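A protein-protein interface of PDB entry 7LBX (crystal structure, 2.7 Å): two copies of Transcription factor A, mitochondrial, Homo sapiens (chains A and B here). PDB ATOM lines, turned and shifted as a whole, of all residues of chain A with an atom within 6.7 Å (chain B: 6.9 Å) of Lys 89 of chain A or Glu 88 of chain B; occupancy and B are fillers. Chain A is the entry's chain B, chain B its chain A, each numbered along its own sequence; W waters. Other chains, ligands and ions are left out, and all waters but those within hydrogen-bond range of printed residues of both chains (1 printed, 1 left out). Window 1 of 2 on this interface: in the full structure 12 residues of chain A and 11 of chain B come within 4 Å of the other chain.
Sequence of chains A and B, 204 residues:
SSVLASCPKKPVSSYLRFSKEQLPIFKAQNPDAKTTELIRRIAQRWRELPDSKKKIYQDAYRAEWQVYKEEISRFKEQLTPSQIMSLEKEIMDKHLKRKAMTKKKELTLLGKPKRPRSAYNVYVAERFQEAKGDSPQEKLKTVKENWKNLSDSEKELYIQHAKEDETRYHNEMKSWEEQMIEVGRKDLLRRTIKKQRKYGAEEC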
ATOM      1  N   ILE A  84       7.077 -18.947   6.131  1.00  0.00           N
ATOM      2  CA  ILE A  84       7.284 -20.356   5.838  1.00  0.00           C
ATOM      3  C   ILE A  84       8.712 -20.691   6.137  1.00  0.00           C
ATOM      4  O   ILE A  84       8.984 -21.677   6.821  1.00  0.00           O
ATOM      5  CB  ILE A  84       6.953 -20.691   4.373  1.00  0.00           C
ATOM      6  CG1 ILE A  84       5.428 -20.611   4.145  1.00  0.00           C
ATOM      7  CG2 ILE A  84       7.522 -22.075   3.997  1.00  0.00           C
ATOM      8  CD1 ILE A  84       5.035 -20.790   2.803  1.00  0.00           C
ATOM      9  N   MET A  85       9.627 -19.894   5.588  1.00  0.00           N
ATOM     10  CA  MET A  85      11.047 -20.105   5.771  1.00  0.00           C
ATOM     11  C   MET A  85      11.452 -19.982   7.244  1.00  0.00           C
ATOM     12  O   MET A  85      12.263 -20.769   7.713  1.00  0.00           O
ATOM     13  CB  MET A  85      11.817 -19.156   4.850  1.00  0.00           C
ATOM     14  CG  MET A  85      13.294 -19.437   4.813  1.00  0.00           C
ATOM     15  SD  MET A  85      14.162 -18.503   3.539  1.00  0.00           S
ATOM     16  CE  MET A  85      15.590 -19.698   3.105  1.00  0.00           C
ATOM     17  N   SER A  86      10.862 -19.036   7.978  1.00  0.00           N
ATOM     18  CA  SER A  86      11.092 -18.864   9.415  1.00  0.00           C
ATOM     19  C   SER A  86      10.626 -20.089  10.163  1.00  0.00           C
ATOM     20  O   SER A  86      11.357 -20.547  11.006  1.00  0.00           O
ATOM     21  CB  SER A  86      10.343 -17.650   9.959  1.00  0.00           C
ATOM     22  OG  SER A  86      10.394 -17.639  11.378  1.00  0.00           O
ATOM     23  N   LEU A  87       9.415 -20.616   9.883  1.00  0.00           N
ATOM     24  CA  LEU A  87       8.875 -21.813  10.558  1.00  0.00           C
ATOM     25  C   LEU A  87       9.794 -23.025  10.384  1.00  0.00           C
ATOM     26  O   LEU A  87      10.071 -23.740  11.349  1.00  0.00           O
ATOM     27  CB  LEU A  87       7.499 -22.141   9.972  1.00  0.00           C
ATOM     28  CG  LEU A  87       6.798 -23.376  10.509  1.00  0.00           C
ATOM     29  CD1 LEU A  87       6.696 -23.323  12.020  1.00  0.00           C
ATOM     30  CD2 LEU A  87       5.446 -23.494   9.880  1.00  0.00           C
ATOM     31  N   GLU A  88      10.236 -23.265   9.131  1.00  0.00           N
ATOM     32  CA  GLU A  88      11.186 -24.330   8.793  1.00  0.00           C
ATOM     33  C   GLU A  88      12.498 -24.174   9.578  1.00  0.00           C
ATOM     34  O   GLU A  88      13.071 -25.169  10.032  1.00  0.00           O
ATOM     35  CB  GLU A  88      11.490 -24.315   7.288  1.00  0.00           C
ATOM     36  CG  GLU A  88      10.376 -24.872   6.428  1.00  0.00           C
ATOM     37  CD  GLU A  88      10.643 -24.874   4.925  1.00  0.00           C
ATOM     38  OE1 GLU A  88      11.813 -24.710   4.497  1.00  0.00           O
ATOM     39  OE2 GLU A  88       9.662 -25.044   4.166  1.00  0.00           O
ATOM     40  N   LYS A  89      12.964 -22.926   9.722  1.00  0.00           N
ATOM     41  CA  LYS A  89      14.183 -22.624  10.457  1.00  0.00           C
ATOM     42  C   LYS A  89      13.960 -22.866  11.946  1.00  0.00           C
ATOM     43  O   LYS A  89      14.862 -23.360  12.608  1.00  0.00           O
ATOM     44  CB  LYS A  89      14.641 -21.156  10.202  1.00  0.00           C
ATOM     45  CG  LYS A  89      15.986 -20.826  10.831  1.00  0.00           C
ATOM     46  CD  LYS A  89      16.398 -19.372  10.684  1.00  0.00           C
ATOM     47  CE  LYS A  89      17.198 -18.851  11.866  1.00  0.00           C
ATOM     48  NZ  LYS A  89      18.413 -19.661  12.135  1.00  0.00           N
ATOM     49  N   GLU A  90      12.766 -22.517  12.465  1.00  0.00           N
ATOM     50  CA  GLU A  90      12.448 -22.676  13.893  1.00  0.00           C
ATOM     51  C   GLU A  90      12.385 -24.133  14.306  1.00  0.00           C
ATOM     52  O   GLU A  90      12.903 -24.499  15.353  1.00  0.00           O
ATOM     53  CB  GLU A  90      11.155 -21.968  14.258  1.00  0.00           C
ATOM     54  CG  GLU A  90      11.273 -20.454  14.261  1.00  0.00           C
ATOM     55  CD  GLU A  90       9.914 -19.800  14.410  1.00  0.00           C
ATOM     56  OE1 GLU A  90       9.482 -19.064  13.490  1.00  0.00           O
ATOM     57  OE2 GLU A  90       9.254 -20.081  15.436  1.00  0.00           O
ATOM     58  N   ILE A  91      11.783 -24.959  13.457  1.00  0.00           N
ATOM     59  CA  ILE A  91      11.695 -26.403  13.653  1.00  0.00           C
ATOM     60  C   ILE A  91      13.098 -27.007  13.687  1.00  0.00           C
ATOM     61  O   ILE A  91      13.436 -27.703  14.649  1.00  0.00           O
ATOM     62  CB  ILE A  91      10.803 -27.031  12.547  1.00  0.00           C
ATOM     63  CG1 ILE A  91       9.321 -26.655  12.802  1.00  0.00           C
ATOM     64  CG2 ILE A  91      10.980 -28.555  12.492  1.00  0.00           C
ATOM     65  CD1 ILE A  91       8.379 -26.862  11.624  1.00  0.00           C
ATOM     66  N   MET A  92      13.925 -26.719  12.666  1.00  0.00           N
ATOM     67  CA  MET A  92      15.284 -27.247  12.623  1.00  0.00           C
ATOM     68  C   MET A  92      16.126 -26.702  13.771  1.00  0.00           C
ATOM     69  O   MET A  92      16.876 -27.461  14.375  1.00  0.00           O
ATOM     70  CB  MET A  92      15.945 -26.941  11.270  1.00  0.00           C
ATOM     71  CG  MET A  92      17.257 -27.716  11.021  1.00  0.00           C
ATOM     72  SD  MET A  92      17.183 -29.552  11.211  1.00  0.00           S
ATOM     73  CE  MET A  92      15.962 -29.954   9.914  1.00  0.00           C
ATOM     74  N   ASP A  93      15.981 -25.421  14.118  1.00  0.00           N
ATOM     75  CA  ASP A  93      16.718 -24.862  15.256  1.00  0.00           C
ATOM     76  C   ASP A  93      16.365 -25.573  16.565  1.00  0.00           C
ATOM     77  O   ASP A  93      17.245 -25.763  17.402  1.00  0.00           O
ATOM     78  CB  ASP A  93      16.442 -23.359  15.433  1.00  0.00           C
ATOM     79  CG  ASP A  93      17.269 -22.437  14.570  1.00  0.00           C
ATOM     80  OD1 ASP A  93      18.096 -22.946  13.768  1.00  0.00           O
ATOM     81  OD2 ASP A  93      17.127 -21.200  14.722  1.00  0.00           O
ATOM     82  N   LYS A  94      15.084 -25.926  16.759  1.00  0.00           N
ATOM     83  CA  LYS A  94      14.634 -26.601  17.969  1.00  0.00           C
ATOM     84  C   LYS A  94      15.254 -27.988  18.000  1.00  0.00           C
ATOM     85  O   LYS A  94      15.839 -28.386  19.012  1.00  0.00           O
ATOM     86  CB  LYS A  94      13.105 -26.675  18.013  1.00  0.00           C
ATOM     87  CG  LYS A  94      12.517 -27.304  19.270  1.00  0.00           C
ATOM     88  CD  LYS A  94      10.987 -27.201  19.310  1.00  0.00           C
ATOM     89  CE  LYS A  94      10.302 -28.532  19.526  1.00  0.00           C
ATOM     90  NZ  LYS A  94       8.821 -28.431  19.465  1.00  0.00           N
ATOM     91  N   GLN B  83      16.081 -11.503   5.605  1.00  0.00           N
ATOM     92  CA  GLN B  83      17.302 -11.866   4.895  1.00  0.00           C
ATOM     93  C   GLN B  83      18.364 -12.373   5.859  1.00  0.00           C
ATOM     94  O   GLN B  83      19.103 -13.294   5.514  1.00  0.00           O
ATOM     95  CB  GLN B  83      17.835 -10.693   4.099  1.00  0.00           C
ATOM     96  CG  GLN B  83      16.865 -10.226   3.018  1.00  0.00           C
ATOM     97  CD  GLN B  83      17.425  -9.111   2.210  1.00  0.00           C
ATOM     98  OE1 GLN B  83      18.246  -8.323   2.678  1.00  0.00           O
ATOM     99  NE2 GLN B  83      17.036  -9.055   0.948  1.00  0.00           N
ATOM    100  N   ILE B  84      18.431 -11.815   7.070  1.00  0.00           N
ATOM    101  CA  ILE B  84      19.375 -12.291   8.052  1.00  0.00           C
ATOM    102  C   ILE B  84      19.005 -13.703   8.381  1.00  0.00           C
ATOM    103  O   ILE B  84      19.887 -14.559   8.373  1.00  0.00           O
ATOM    104  CB  ILE B  84      19.378 -11.425   9.325  1.00  0.00           C
ATOM    105  CG1 ILE B  84      20.029 -10.053   9.037  1.00  0.00           C
ATOM    106  CG2 ILE B  84      20.102 -12.152  10.471  1.00  0.00           C
ATOM    107  CD1 ILE B  84      19.950  -9.158  10.117  1.00  0.00           C
ATOM    108  N   MET B  85      17.700 -13.984   8.680  1.00  0.00           N
ATOM    109  CA  MET B  85      17.321 -15.360   9.024  1.00  0.00           C
ATOM    110  C   MET B  85      17.471 -16.290   7.815  1.00  0.00           C
ATOM    111  O   MET B  85      17.954 -17.408   7.977  1.00  0.00           O
ATOM    112  CB  MET B  85      15.944 -15.459   9.714  1.00  0.00           C
ATOM    113  CG  MET B  85      14.761 -15.546   8.794  1.00  0.00           C
ATOM    114  SD  MET B  85      14.334 -17.178   8.114  1.00  0.00           S
ATOM    115  CE  MET B  85      13.291 -16.621   6.766  1.00  0.00           C
ATOM    116  N   SER B  86      17.159 -15.813   6.607  1.00  0.00           N
ATOM    117  CA  SER B  86      17.359 -16.620   5.403  1.00  0.00           C
ATOM    118  C   SER B  86      18.829 -17.000   5.266  1.00  0.00           C
ATOM    119  O   SER B  86      19.100 -18.164   5.006  1.00  0.00           O
ATOM    120  CB  SER B  86      16.934 -15.863   4.156  1.00  0.00           C
ATOM    121  OG  SER B  86      17.329 -16.569   2.990  1.00  0.00           O
ATOM    122  N   LEU B  87      19.776 -16.034   5.442  1.00  0.00           N
ATOM    123  CA  LEU B  87      21.216 -16.307   5.356  1.00  0.00           C
ATOM    124  C   LEU B  87      21.646 -17.366   6.377  1.00  0.00           C
ATOM    125  O   LEU B  87      22.380 -18.299   6.041  1.00  0.00           O
ATOM    126  CB  LEU B  87      21.996 -15.018   5.596  1.00  0.00           C
ATOM    127  CG  LEU B  87      23.522 -15.102   5.586  1.00  0.00           C
ATOM    128  CD1 LEU B  87      24.023 -15.739   4.321  1.00  0.00           C
ATOM    129  CD2 LEU B  87      24.127 -13.717   5.764  1.00  0.00           C
ATOM    130  N   GLU B  88      21.202 -17.193   7.631  1.00  0.00           N
ATOM    131  CA  GLU B  88      21.445 -18.127   8.728  1.00  0.00           C
ATOM    132  C   GLU B  88      20.896 -19.507   8.396  1.00  0.00           C
ATOM    133  O   GLU B  88      21.538 -20.498   8.714  1.00  0.00           O
ATOM    134  CB  GLU B  88      20.806 -17.644  10.035  1.00  0.00           C
ATOM    135  CG  GLU B  88      21.583 -16.521  10.695  1.00  0.00           C
ATOM    136  CD  GLU B  88      21.064 -15.984  12.013  1.00  0.00           C
ATOM    137  OE1 GLU B  88      21.815 -15.189  12.623  1.00  0.00           O
ATOM    138  OE2 GLU B  88      19.939 -16.340  12.443  1.00  0.00           O
ATOM    139  N   LYS B  89      19.727 -19.573   7.759  1.00  0.00           N
ATOM    140  CA  LYS B  89      19.110 -20.834   7.363  1.00  0.00           C
ATOM    141  C   LYS B  89      19.911 -21.508   6.241  1.00  0.00           C
ATOM    142  O   LYS B  89      20.063 -22.732   6.301  1.00  0.00           O
ATOM    143  CB  LYS B  89      17.635 -20.626   6.920  1.00  0.00           C
ATOM    144  CG  LYS B  89      16.899 -21.933   6.639  1.00  0.00           C
ATOM    145  CD  LYS B  89      15.494 -21.749   6.093  1.00  0.00           C
ATOM    146  CE  LYS B  89      15.083 -22.867   5.148  1.00  0.00           C
ATOM    147  NZ  LYS B  89      15.177 -24.208   5.771  1.00  0.00           N
ATOM    148  N   GLU B  90      20.380 -20.770   5.188  1.00  0.00           N
ATOM    149  CA  GLU B  90      21.157 -21.403   4.093  1.00  0.00           C
ATOM    150  C   GLU B  90      22.480 -21.905   4.613  1.00  0.00           C
ATOM    151  O   GLU B  90      22.885 -22.998   4.218  1.00  0.00           O
ATOM    152  CB  GLU B  90      21.439 -20.456   2.931  1.00  0.00           C
ATOM    153  CG  GLU B  90      20.217 -19.949   2.202  1.00  0.00           C
ATOM    154  CD  GLU B  90      20.501 -18.759   1.313  1.00  0.00           C
ATOM    155  OE1 GLU B  90      20.001 -17.644   1.606  1.00  0.00           O
ATOM    156  OE2 GLU B  90      21.258 -18.944   0.333  1.00  0.00           O
ATOM    157  N   ILE B  91      23.162 -21.126   5.508  1.00  0.00           N
ATOM    158  CA  ILE B  91      24.420 -21.575   6.098  1.00  0.00           C
ATOM    159  C   ILE B  91      24.197 -22.901   6.845  1.00  0.00           C
ATOM    160  O   ILE B  91      24.895 -23.868   6.576  1.00  0.00           O
ATOM    161  CB  ILE B  91      25.024 -20.483   7.014  1.00  0.00           C
ATOM    162  CG1 ILE B  91      25.561 -19.314   6.170  1.00  0.00           C
ATOM    163  CG2 ILE B  91      26.123 -21.037   7.941  1.00  0.00           C
ATOM    164  CD1 ILE B  91      25.828 -18.022   6.943  1.00  0.00           C
ATOM    165  N   MET B  92      23.219 -22.954   7.760  1.00  0.00           N
ATOM    166  CA  MET B  92      22.928 -24.160   8.538  1.00  0.00           C
ATOM    167  C   MET B  92      22.466 -25.288   7.641  1.00  0.00           C
ATOM    168  O   MET B  92      22.912 -26.418   7.828  1.00  0.00           O
ATOM    169  CB  MET B  92      21.899 -23.884   9.641  1.00  0.00           C
ATOM    170  CG  MET B  92      21.779 -24.987  10.692  1.00  0.00           C
ATOM    171  SD  MET B  92      23.354 -25.507  11.498  1.00  0.00           S
ATOM    172  CE  MET B  92      23.829 -23.986  12.329  1.00  0.00           C
ATOM    173  N   ASP B  93      21.635 -25.009   6.636  1.00  0.00           N
ATOM    174  CA  ASP B  93      21.223 -26.066   5.700  1.00  0.00           C
ATOM    175  C   ASP B  93      22.414 -26.675   4.964  1.00  0.00           C
ATOM    176  O   ASP B  93      22.428 -27.882   4.731  1.00  0.00           O
ATOM    177  CB  ASP B  93      20.218 -25.528   4.658  1.00  0.00           C
ATOM    178  CG  ASP B  93      18.765 -25.469   5.093  1.00  0.00           C
ATOM    179  OD1 ASP B  93      18.470 -25.837   6.259  1.00  0.00           O
ATOM    180  OD2 ASP B  93      17.916 -25.084   4.262  1.00  0.00           O
HETATM  181  O   HOH W   1      15.834 -25.821   8.045  1.00  0.00           O
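The side-chain carboxylate of Glu 90 of chain B is in hydrogen-bond range of the side-chain hydroxyl of Ser 86 of chain B (3.2 Å).
The side-chain amino group (NZ) of Lys 89 of chain B lies within salt-bridge range of the side-chain carboxylate (OD2) of Asp 93 of chain B.
The side-chain amino group (NZ) of Lys 89 of chain A lies within salt-bridge range of the side-chain carboxylate (OD2) of Asp 93 of chain A (3.3 Å).
OG of Ser 86 of chain A sits at hydrogen-bond distance from OE1 of Glu 90 of chain A (2.7 Å).
OG of Ser 86 of chain B lies close to SD of Met 85 of chain A (3.8 Å).
The side-chain amino group of Lys 89 of chain A is in salt-bridge range of the side-chain carboxylate of Glu 88 of chain B, at 3.7 Å.
The side-chain amino group (NZ) of Lys 89 of chain B lies within salt-bridge range of the side-chain carboxylate (OE1) of Glu 88 of chain A, at 3.6 Å.
Met 85 of chain A touches its own counterpart, Met 85 of chain B.
Met 85 of chain A touches Ser 86 of chain B, and with the chains exchanged Ser 86 of chain A touches Met 85 of chain B.
Met 85 of chain A touches Lys 89 of chain B, and with the chains exchanged Lys 89 of chain A touches Met 85 of chain B.
Glu 88 of chain A touches Lys 89 of chain B, and with the chains exchanged Lys 89 of chain A touches Glu 88 of chain B.
10 positions are printed for both chains.
Of the 7 pairs that touch across the chains among the printed residues, 7 have their exchanged pair printed and touching as well.
Water W1 lies within hydrogen-bond range of the side-chain amino group of Lys 89 of chain B (2.9 Å), the side-chain carboxylate of Asp 93 of chain B (3.2 Å) and the backbone carbonyl oxygen of Glu 88 of chain A (3.5 Å).
Met 85 of chain A touches Met 85 of chain B (CG to CE, 3.4 Å).
Met 85 of chain A touches Lys 89 of chain B.
N of Ser 86 of chain A touches CE of Met 85 of chain B, 3.6 Å away.
CD of Lys 89 of chain A touches O of Met 85 of chain B (3.7 Å).
Of chain B, only Met 85 and Glu 88 come within 4 Å of Lys 89 of chain A.
Glu 88 of chain B touches just one residue of chain A: Lys 89.
Of the printed residues of chain A, Met 85 of chain B touches Met 85, Ser 86 and Lys 89.
Of the printed residues of chain A, Lys 89 of chain B touches Met 85 and Glu 88.
Of the printed residues of chain B, Ser 86 of chain A touches Met 85 (3.6 Å).
Printed residues of chain A within 4 Å of Ser 86 of chain B: Met 85 (3.6 Å).
Of the printed residues of chain B, Glu 88 of chain A touches Lys 89.
Glu 90 of chain A touches none of the printed residues of chain B.
The nearest residue of chain A that does not touch Glu 88 of chain B is Asp 93 of chain A (6.1 Å).
Printed residues of chain A that touch a printed residue of chain B: Met 85, Ser 86, Glu 88 and Lys 89.
Hydrophobic or aromatic side chains of chain A within 4 Å of the printed part of chain B: Met 85.
Hydrophobic or aromatic side chains of chain B within 4 Å of the printed part of chain A: Met 85.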
